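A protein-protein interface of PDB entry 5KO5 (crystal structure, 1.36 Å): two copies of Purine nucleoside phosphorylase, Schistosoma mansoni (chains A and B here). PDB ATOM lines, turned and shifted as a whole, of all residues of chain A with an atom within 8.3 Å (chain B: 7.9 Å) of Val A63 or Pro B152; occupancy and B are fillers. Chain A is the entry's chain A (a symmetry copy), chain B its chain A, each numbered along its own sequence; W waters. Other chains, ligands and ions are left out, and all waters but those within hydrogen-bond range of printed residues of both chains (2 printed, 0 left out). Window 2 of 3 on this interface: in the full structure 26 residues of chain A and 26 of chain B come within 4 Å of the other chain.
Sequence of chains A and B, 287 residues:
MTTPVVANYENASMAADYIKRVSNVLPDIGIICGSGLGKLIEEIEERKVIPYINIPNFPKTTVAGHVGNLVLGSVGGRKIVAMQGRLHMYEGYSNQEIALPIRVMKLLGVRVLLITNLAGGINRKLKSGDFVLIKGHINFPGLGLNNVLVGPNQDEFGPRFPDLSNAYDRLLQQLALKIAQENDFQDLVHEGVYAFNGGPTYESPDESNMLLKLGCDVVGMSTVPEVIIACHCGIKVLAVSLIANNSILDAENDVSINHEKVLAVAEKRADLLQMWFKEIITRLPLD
Of the 14 printed residues of chain B, 5 touch a printed residue of chain A.
Hydrophobic or aromatic side chains of chain A within 4 Å of the printed part of chain B: Val A63 and Pro A200.
Among the printed residues, 11 pairs touch across the chains.
Among the printed residues, Asp or Glu carboxylates within 4 Å of a Lys or Arg side-chain nitrogen of the other chain: Glu A91 with Arg B160 (2.9 Å).
Water W2 lies within hydrogen-bond range of OE1 of Glu A91 (2.8 Å) and N of Asn B153 (2.8 Å).
Water W1 bridges O of Val A63 and O of Asn B153.
Val A63 touches just one residue of chain B: Pro B152.
Pro B152 touches just these residues of chain A: Val A63 (3.6 Å) and Glu A91 (3.5 Å).
Gly B151 touches just these residues of chain A: Tyr A90, Glu A91 and Gly A92.
Of the printed residues of chain B, Pro A200 touches Leu B149 (3.6 Å), Val B150 (3.9 Å) and Arg B160 (3.4 Å).
Printed residues of chain B within 4 Å of Met A89: Val B150 (3.9 Å).
Of the printed residues of chain A, Arg B160 touches Glu A91 and Pro A200.
The nearest residue of chain A that does not touch Pro B152 is Tyr A90 (5.2 Å).
The nearest printed residue of chain A that does not touch Arg B160 is Tyr A90 (4.003 Å).
N of Gly B151 lies within hydrogen-bond range of O of Tyr A90, 2.9 Å away.
NH2 of Arg B160 is in salt-bridge range of OE2 of Glu A91.
The backbone carbonyl oxygen (O) of Glu A91 sits close to the backbone nitrogen (N) of Pro B152 (3.5 Å).
No position is printed for both chains.
Of the 11 pairs that touch across the chains among the printed residues, none has its exchanged pair printed and touching as well.
The guanidinium group (NH1) of Arg B160 sits at hydrogen-bond distance from the backbone carbonyl oxygen (O) of Leu B149.
The backbone carbonyl oxygen of Gly B151 sits at hydrogen-bond distance from the guanidinium group of Arg B160 (2.9 Å).
CG1 of Val A63 touches CB of Pro B152 (3.6 Å).
O of Met A89 touches CG1 of Val B150, 3.9 Å away.
O of Tyr A90 touches CA of Val B150, 3.4 Å away.
Gly B151 touches Glu A91 (C to O, 3.3 Å).
N of Gly B151 touches N of Gly A92, 3.96 Å away.
Pro A200 touches Leu B149 (CG to CB, 3.6 Å).
Pro A200 touches Val B150 (CD to N, 3.9 Å).
Pro A200 touches Arg B160.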
ATOM      1  N   LYS A  60     -11.340  -3.118   2.614  1.00  0.00           N
ATOM      2  CA  LYS A  60     -12.151  -2.110   1.947  1.00  0.00           C
ATOM      3  C   LYS A  60     -11.336  -0.831   1.777  1.00  0.00           C
ATOM      4  O   LYS A  60     -10.767  -0.316   2.741  1.00  0.00           O
ATOM      5  CB  LYS A  60     -13.389  -1.825   2.796  1.00  0.00           C
ATOM      6  CG  LYS A  60     -14.338  -0.785   2.215  1.00  0.00           C
ATOM      7  CD  LYS A  60     -15.633  -0.732   3.020  1.00  0.00           C
ATOM      8  CE  LYS A  60     -16.620   0.261   2.434  1.00  0.00           C
ATOM      9  NZ  LYS A  60     -17.016  -0.103   1.045  1.00  0.00           N
ATOM     10  N   THR A  61     -11.279  -0.313   0.547  1.00  0.00           N
ATOM     11  CA  THR A  61     -10.477   0.870   0.244  1.00  0.00           C
ATOM     12  C   THR A  61     -11.303   2.007  -0.353  1.00  0.00           C
ATOM     13  O   THR A  61     -10.729   2.951  -0.907  1.00  0.00           O
ATOM     14  CB  THR A  61      -9.318   0.524  -0.694  1.00  0.00           C
ATOM     15  OG1 THR A  61      -9.836   0.165  -1.981  1.00  0.00           O
ATOM     16  CG2 THR A  61      -8.509  -0.641  -0.152  1.00  0.00           C
ATOM     17  N   THR A  62     -12.632   1.949  -0.249  1.00  0.00           N
ATOM     18  CA  THR A  62     -13.455   2.942  -0.932  1.00  0.00           C
ATOM     19  C   THR A  62     -13.429   4.305  -0.245  1.00  0.00           C
ATOM     20  O   THR A  62     -13.673   5.323  -0.901  1.00  0.00           O
ATOM     21  CB  THR A  62     -14.887   2.428  -1.078  1.00  0.00           C
ATOM     22  OG1 THR A  62     -15.427   2.150   0.218  1.00  0.00           O
ATOM     23  CG2 THR A  62     -14.907   1.151  -1.911  1.00  0.00           C
ATOM     24  N   VAL A  63     -13.149   4.367   1.058  1.00  0.00           N
ATOM     25  CA  VAL A  63     -13.069   5.676   1.704  1.00  0.00           C
ATOM     26  C   VAL A  63     -11.920   6.487   1.114  1.00  0.00           C
ATOM     27  O   VAL A  63     -12.079   7.661   0.761  1.00  0.00           O
ATOM     28  CB  VAL A  63     -12.975   5.543   3.234  1.00  0.00           C
ATOM     29  CG1 VAL A  63     -12.777   6.910   3.860  1.00  0.00           C
ATOM     30  CG2 VAL A  63     -14.241   4.903   3.795  1.00  0.00           C
ATOM     31  N   ALA A  64     -10.746   5.863   0.977  1.00  0.00           N
ATOM     32  CA  ALA A  64      -9.645   6.537   0.295  1.00  0.00           C
ATOM     33  C   ALA A  64      -9.909   6.654  -1.198  1.00  0.00           C
ATOM     34  O   ALA A  64      -9.442   7.605  -1.839  1.00  0.00           O
ATOM     35  CB  ALA A  64      -8.338   5.784   0.541  1.00  0.00           C
ATOM     36  N   GLY A  65     -10.657   5.710  -1.764  1.00  0.00           N
ATOM     37  CA  GLY A  65     -10.921   5.721  -3.185  1.00  0.00           C
ATOM     38  C   GLY A  65      -9.676   5.382  -3.988  1.00  0.00           C
ATOM     39  O   GLY A  65      -8.715   4.785  -3.492  1.00  0.00           O
ATOM     40  N   HIS A  66      -9.711   5.782  -5.259  1.00  0.00           N
ATOM     41  CA  HIS A  66      -8.635   5.531  -6.214  1.00  0.00           C
ATOM     42  C   HIS A  66      -8.470   4.039  -6.500  1.00  0.00           C
ATOM     43  O   HIS A  66      -9.248   3.216  -6.007  1.00  0.00           O
ATOM     44  CB  HIS A  66      -7.330   6.217  -5.780  1.00  0.00           C
ATOM     45  CG  HIS A  66      -7.477   7.691  -5.543  1.00  0.00           C
ATOM     46  ND1 HIS A  66      -7.338   8.625  -6.547  1.00  0.00           N
ATOM     47  CD2 HIS A  66      -7.762   8.389  -4.417  1.00  0.00           C
ATOM     48  CE1 HIS A  66      -7.528   9.835  -6.050  1.00  0.00           C
ATOM     49  NE2 HIS A  66      -7.784   9.719  -4.759  1.00  0.00           N
ATOM     50  N   MET A  89      -0.490   3.134   5.909  1.00  0.00           N
ATOM     51  CA  MET A  89      -1.025   3.154   7.267  1.00  0.00           C
ATOM     52  C   MET A  89      -1.531   4.535   7.672  1.00  0.00           C
ATOM     53  O   MET A  89      -2.438   4.621   8.507  1.00  0.00           O
ATOM     54  CB  MET A  89      -0.025   2.530   8.250  1.00  0.00           C
ATOM     55  CG  MET A  89       0.270   1.074   7.850  1.00  0.00           C
ATOM     56  SD  MET A  89       0.817  -0.018   9.176  1.00  0.00           S
ATOM     57  CE  MET A  89      -0.653  -0.099  10.187  1.00  0.00           C
ATOM     58  N   TYR A  90      -1.024   5.606   7.058  1.00  0.00           N
ATOM     59  CA  TYR A  90      -1.561   6.929   7.379  1.00  0.00           C
ATOM     60  C   TYR A  90      -3.009   7.084   6.945  1.00  0.00           C
ATOM     61  O   TYR A  90      -3.653   8.048   7.368  1.00  0.00           O
ATOM     62  CB  TYR A  90      -0.696   8.068   6.809  1.00  0.00           C
ATOM     63  CG  TYR A  90      -0.464   7.988   5.317  1.00  0.00           C
ATOM     64  CD1 TYR A  90      -1.494   8.226   4.412  1.00  0.00           C
ATOM     65  CD2 TYR A  90       0.787   7.675   4.814  1.00  0.00           C
ATOM     66  CE1 TYR A  90      -1.284   8.131   3.045  1.00  0.00           C
ATOM     67  CE2 TYR A  90       1.005   7.580   3.453  1.00  0.00           C
ATOM     68  CZ  TYR A  90      -0.033   7.814   2.577  1.00  0.00           C
ATOM     69  OH  TYR A  90       0.196   7.701   1.228  1.00  0.00           O
ATOM     70  N   GLU A  91      -3.528   6.195   6.095  1.00  0.00           N
ATOM     71  CA  GLU A  91      -4.945   6.247   5.745  1.00  0.00           C
ATOM     72  C   GLU A  91      -5.841   5.714   6.849  1.00  0.00           C
ATOM     73  O   GLU A  91      -7.061   5.899   6.778  1.00  0.00           O
ATOM     74  CB  GLU A  91      -5.227   5.427   4.487  1.00  0.00           C
ATOM     75  CG  GLU A  91      -4.695   6.038   3.235  1.00  0.00           C
ATOM     76  CD  GLU A  91      -5.446   7.313   2.801  1.00  0.00           C
ATOM     77  OE1 GLU A  91      -6.641   7.515   3.142  1.00  0.00           O
ATOM     78  OE2 GLU A  91      -4.826   8.100   2.082  1.00  0.00           O
ATOM     79  N   GLY A  92      -5.272   5.049   7.847  1.00  0.00           N
ATOM     80  CA  GLY A  92      -6.036   4.459   8.921  1.00  0.00           C
ATOM     81  C   GLY A  92      -6.255   2.971   8.802  1.00  0.00           C
ATOM     82  O   GLY A  92      -6.950   2.402   9.651  1.00  0.00           O
ATOM     83  N   TYR A  93      -5.677   2.322   7.793  1.00  0.00           N
ATOM     84  CA  TYR A  93      -5.804   0.872   7.690  1.00  0.00           C
ATOM     85  C   TYR A  93      -5.197   0.193   8.909  1.00  0.00           C
ATOM     86  O   TYR A  93      -4.149   0.607   9.418  1.00  0.00           O
ATOM     87  CB  TYR A  93      -5.088   0.365   6.438  1.00  0.00           C
ATOM     88  CG  TYR A  93      -5.732   0.824   5.162  1.00  0.00           C
ATOM     89  CD1 TYR A  93      -7.026   0.444   4.850  1.00  0.00           C
ATOM     90  CD2 TYR A  93      -5.054   1.639   4.272  1.00  0.00           C
ATOM     91  CE1 TYR A  93      -7.635   0.878   3.688  1.00  0.00           C
ATOM     92  CE2 TYR A  93      -5.645   2.067   3.111  1.00  0.00           C
ATOM     93  CZ  TYR A  93      -6.929   1.681   2.816  1.00  0.00           C
ATOM     94  OH  TYR A  93      -7.528   2.116   1.657  1.00  0.00           O
ATOM     95  N   PRO A 200       0.551  11.536   7.979  1.00  0.00           N
ATOM     96  CA  PRO A 200       0.851  11.881   6.579  1.00  0.00           C
ATOM     97  C   PRO A 200       1.475  13.260   6.403  1.00  0.00           C
ATOM     98  O   PRO A 200       1.693  13.671   5.259  1.00  0.00           O
ATOM     99  CB  PRO A 200      -0.532  11.864   5.932  1.00  0.00           C
ATOM    100  CG  PRO A 200      -1.442  12.385   7.057  1.00  0.00           C
ATOM    101  CD  PRO A 200      -0.864  11.778   8.329  1.00  0.00           C
ATOM    102  N   VAL B   6     -17.005  11.982  12.361  1.00  0.00           N
ATOM    103  CA  VAL B   6     -15.840  12.324  11.554  1.00  0.00           C
ATOM    104  C   VAL B   6     -15.723  13.841  11.467  1.00  0.00           C
ATOM    105  O   VAL B   6     -16.731  14.552  11.374  1.00  0.00           O
ATOM    106  CB  VAL B   6     -15.964  11.679  10.163  1.00  0.00           C
ATOM    107  CG1 VAL B   6     -14.757  12.019   9.297  1.00  0.00           C
ATOM    108  CG2 VAL B   6     -16.086  10.174  10.316  1.00  0.00           C
ATOM    109  N   ALA B   7     -14.485  14.344  11.502  1.00  0.00           N
ATOM    110  CA  ALA B   7     -14.215  15.777  11.366  1.00  0.00           C
ATOM    111  C   ALA B   7     -14.243  16.202   9.891  1.00  0.00           C
ATOM    112  O   ALA B   7     -13.268  16.695   9.316  1.00  0.00           O
ATOM    113  CB  ALA B   7     -12.884  16.120  12.024  1.00  0.00           C
ATOM    114  N   GLN B  96     -10.366  12.579  15.179  1.00  0.00           N
ATOM    115  CA  GLN B  96     -11.539  13.303  14.701  1.00  0.00           C
ATOM    116  C   GLN B  96     -12.019  14.325  15.722  1.00  0.00           C
ATOM    117  O   GLN B  96     -12.480  15.415  15.350  1.00  0.00           O
ATOM    118  CB  GLN B  96     -12.669  12.326  14.374  1.00  0.00           C
ATOM    119  CG  GLN B  96     -12.297  11.209  13.405  1.00  0.00           C
ATOM    120  CD  GLN B  96     -11.649  11.715  12.144  1.00  0.00           C
ATOM    121  OE1 GLN B  96     -12.060  12.723  11.568  1.00  0.00           O
ATOM    122  NE2 GLN B  96     -10.622  11.000  11.694  1.00  0.00           N
ATOM    123  N   ARG B 103     -11.384  22.814  12.670  1.00  0.00           N
ATOM    124  CA  ARG B 103     -12.045  22.966  11.379  1.00  0.00           C
ATOM    125  C   ARG B 103     -13.301  23.825  11.478  1.00  0.00           C
ATOM    126  O   ARG B 103     -13.618  24.561  10.534  1.00  0.00           O
ATOM    127  CB  ARG B 103     -12.316  21.587  10.796  1.00  0.00           C
ATOM    128  CG  ARG B 103     -11.006  20.946  10.388  1.00  0.00           C
ATOM    129  CD  ARG B 103     -11.138  19.526   9.855  1.00  0.00           C
ATOM    130  NE  ARG B 103      -9.833  19.113   9.340  1.00  0.00           N
ATOM    131  CZ  ARG B 103      -9.495  17.862   9.064  1.00  0.00           C
ATOM    132  NH1 ARG B 103     -10.376  16.879   9.226  1.00  0.00           N
ATOM    133  NH2 ARG B 103      -8.267  17.597   8.633  1.00  0.00           N
ATOM    134  N   VAL B 148      -2.174  13.325  14.238  1.00  0.00           N
ATOM    135  CA  VAL B 148      -3.571  13.759  14.286  1.00  0.00           C
ATOM    136  C   VAL B 148      -4.276  13.646  12.934  1.00  0.00           C
ATOM    137  O   VAL B 148      -5.511  13.586  12.894  1.00  0.00           O
ATOM    138  CB  VAL B 148      -3.650  15.184  14.882  1.00  0.00           C
ATOM    139  CG1 VAL B 148      -3.089  16.199  13.904  1.00  0.00           C
ATOM    140  CG2 VAL B 148      -5.090  15.537  15.256  1.00  0.00           C
ATOM    141  N   LEU B 149      -3.523  13.590  11.820  1.00  0.00           N
ATOM    142  CA  LEU B 149      -4.128  13.450  10.498  1.00  0.00           C
ATOM    143  C   LEU B 149      -4.239  12.007  10.005  1.00  0.00           C
ATOM    144  O   LEU B 149      -4.749  11.798   8.894  1.00  0.00           O
ATOM    145  CB  LEU B 149      -3.373  14.310   9.463  1.00  0.00           C
ATOM    146  CG  LEU B 149      -3.672  15.809   9.511  1.00  0.00           C
ATOM    147  CD1 LEU B 149      -2.705  16.548   8.590  1.00  0.00           C
ATOM    148  CD2 LEU B 149      -5.131  16.083   9.100  1.00  0.00           C
ATOM    149  N   VAL B 150      -3.801  11.008  10.785  1.00  0.00           N
ATOM    150  CA  VAL B 150      -4.011   9.631  10.347  1.00  0.00           C
ATOM    151  C   VAL B 150      -5.498   9.378  10.179  1.00  0.00           C
ATOM    152  O   VAL B 150      -6.301   9.687  11.071  1.00  0.00           O
ATOM    153  CB  VAL B 150      -3.377   8.645  11.338  1.00  0.00           C
ATOM    154  CG1 VAL B 150      -3.849   7.211  11.030  1.00  0.00           C
ATOM    155  CG2 VAL B 150      -1.871   8.700  11.263  1.00  0.00           C
ATOM    156  N   GLY B 151      -5.865   8.781   9.042  1.00  0.00           N
ATOM    157  CA  GLY B 151      -7.242   8.559   8.670  1.00  0.00           C
ATOM    158  C   GLY B 151      -7.474   9.087   7.272  1.00  0.00           C
ATOM    159  O   GLY B 151      -6.568   9.635   6.634  1.00  0.00           O
ATOM    160  N   PRO B 152      -8.699   8.969   6.772  1.00  0.00           N
ATOM    161  CA  PRO B 152      -9.006   9.544   5.457  1.00  0.00           C
ATOM    162  C   PRO B 152      -8.726  11.037   5.471  1.00  0.00           C
ATOM    163  O   PRO B 152      -8.933  11.710   6.482  1.00  0.00           O
ATOM    164  CB  PRO B 152     -10.502   9.275   5.293  1.00  0.00           C
ATOM    165  CG  PRO B 152     -11.014   9.068   6.697  1.00  0.00           C
ATOM    166  CD  PRO B 152      -9.887   8.395   7.430  1.00  0.00           C
ATOM    167  N   ASN B 153      -8.220  11.555   4.355  1.00  0.00           N
ATOM    168  CA  ASN B 153      -8.079  13.003   4.239  1.00  0.00           C
ATOM    169  C   ASN B 153      -9.423  13.664   3.962  1.00  0.00           C
ATOM    170  O   ASN B 153     -10.239  13.159   3.186  1.00  0.00           O
ATOM    171  CB  ASN B 153      -7.112  13.387   3.122  1.00  0.00           C
ATOM    172  CG  ASN B 153      -6.771  14.869   3.158  1.00  0.00           C
ATOM    173  OD1 ASN B 153      -6.266  15.355   4.166  1.00  0.00           O
ATOM    174  ND2 ASN B 153      -7.054  15.592   2.081  1.00  0.00           N
ATOM    175  N   GLN B 154      -9.636  14.817   4.588  1.00  0.00           N
ATOM    176  CA  GLN B 154     -10.814  15.643   4.327  1.00  0.00           C
ATOM    177  C   GLN B 154     -10.383  16.727   3.341  1.00  0.00           C
ATOM    178  O   GLN B 154      -9.848  17.775   3.719  1.00  0.00           O
ATOM    179  CB  GLN B 154     -11.369  16.202   5.635  1.00  0.00           C
ATOM    180  CG  GLN B 154     -11.704  15.115   6.656  1.00  0.00           C
ATOM    181  CD  GLN B 154     -12.679  14.076   6.129  1.00  0.00           C
ATOM    182  OE1 GLN B 154     -13.494  14.350   5.249  1.00  0.00           O
ATOM    183  NE2 GLN B 154     -12.595  12.864   6.674  1.00  0.00           N
ATOM    184  N   ASP B 155     -10.615  16.447   2.054  1.00  0.00           N
ATOM    185  CA  ASP B 155     -10.042  17.253   0.975  1.00  0.00           C
ATOM    186  C   ASP B 155     -10.505  18.705   1.012  1.00  0.00           C
ATOM    187  O   ASP B 155      -9.767  19.604   0.582  1.00  0.00           O
ATOM    188  CB  ASP B 155     -10.414  16.647  -0.385  1.00  0.00           C
ATOM    189  CG  ASP B 155      -9.846  15.244  -0.583  1.00  0.00           C
ATOM    190  OD1 ASP B 155      -8.720  14.985  -0.131  1.00  0.00           O
ATOM    191  OD2 ASP B 155     -10.526  14.401  -1.210  1.00  0.00           O
ATOM    192  N   ARG B 160      -3.616  15.887   1.298  1.00  0.00           N
ATOM    193  CA  ARG B 160      -3.278  14.619   1.940  1.00  0.00           C
ATOM    194  C   ARG B 160      -1.959  14.709   2.704  1.00  0.00           C
ATOM    195  O   ARG B 160      -1.831  14.158   3.807  1.00  0.00           O
ATOM    196  CB  ARG B 160      -3.234  13.520   0.870  1.00  0.00           C
ATOM    197  CG  ARG B 160      -2.645  12.179   1.336  1.00  0.00           C
ATOM    198  CD  ARG B 160      -3.616  11.338   2.196  1.00  0.00           C
ATOM    199  NE  ARG B 160      -3.779  11.840   3.559  1.00  0.00           N
ATOM    200  CZ  ARG B 160      -4.459  11.206   4.501  1.00  0.00           C
ATOM    201  NH1 ARG B 160      -4.582  11.729   5.713  1.00  0.00           N
ATOM    202  NH2 ARG B 160      -5.075  10.066   4.217  1.00  0.00           N
ATOM    203  N   HIS B 232      -2.942  22.350   8.134  1.00  0.00           N
ATOM    204  CA  HIS B 232      -3.594  21.608   7.065  1.00  0.00           C
ATOM    205  C   HIS B 232      -4.666  22.450   6.374  1.00  0.00           C
ATOM    206  O   HIS B 232      -4.808  22.393   5.146  1.00  0.00           O
ATOM    207  CB  HIS B 232      -4.159  20.316   7.667  1.00  0.00           C
ATOM    208  CG  HIS B 232      -4.928  19.467   6.711  1.00  0.00           C
ATOM    209  ND1 HIS B 232      -6.305  19.482   6.652  1.00  0.00           N
ATOM    210  CD2 HIS B 232      -4.519  18.540   5.814  1.00  0.00           C
ATOM    211  CE1 HIS B 232      -6.710  18.610   5.744  1.00  0.00           C
ATOM    212  NE2 HIS B 232      -5.646  18.032   5.214  1.00  0.00           N
HETATM  213  O   HOH W   1     -10.692  10.341   1.647  1.00  0.00           O
HETATM  214  O   HOH W   2      -7.915   9.832   2.123  1.00  0.00           O
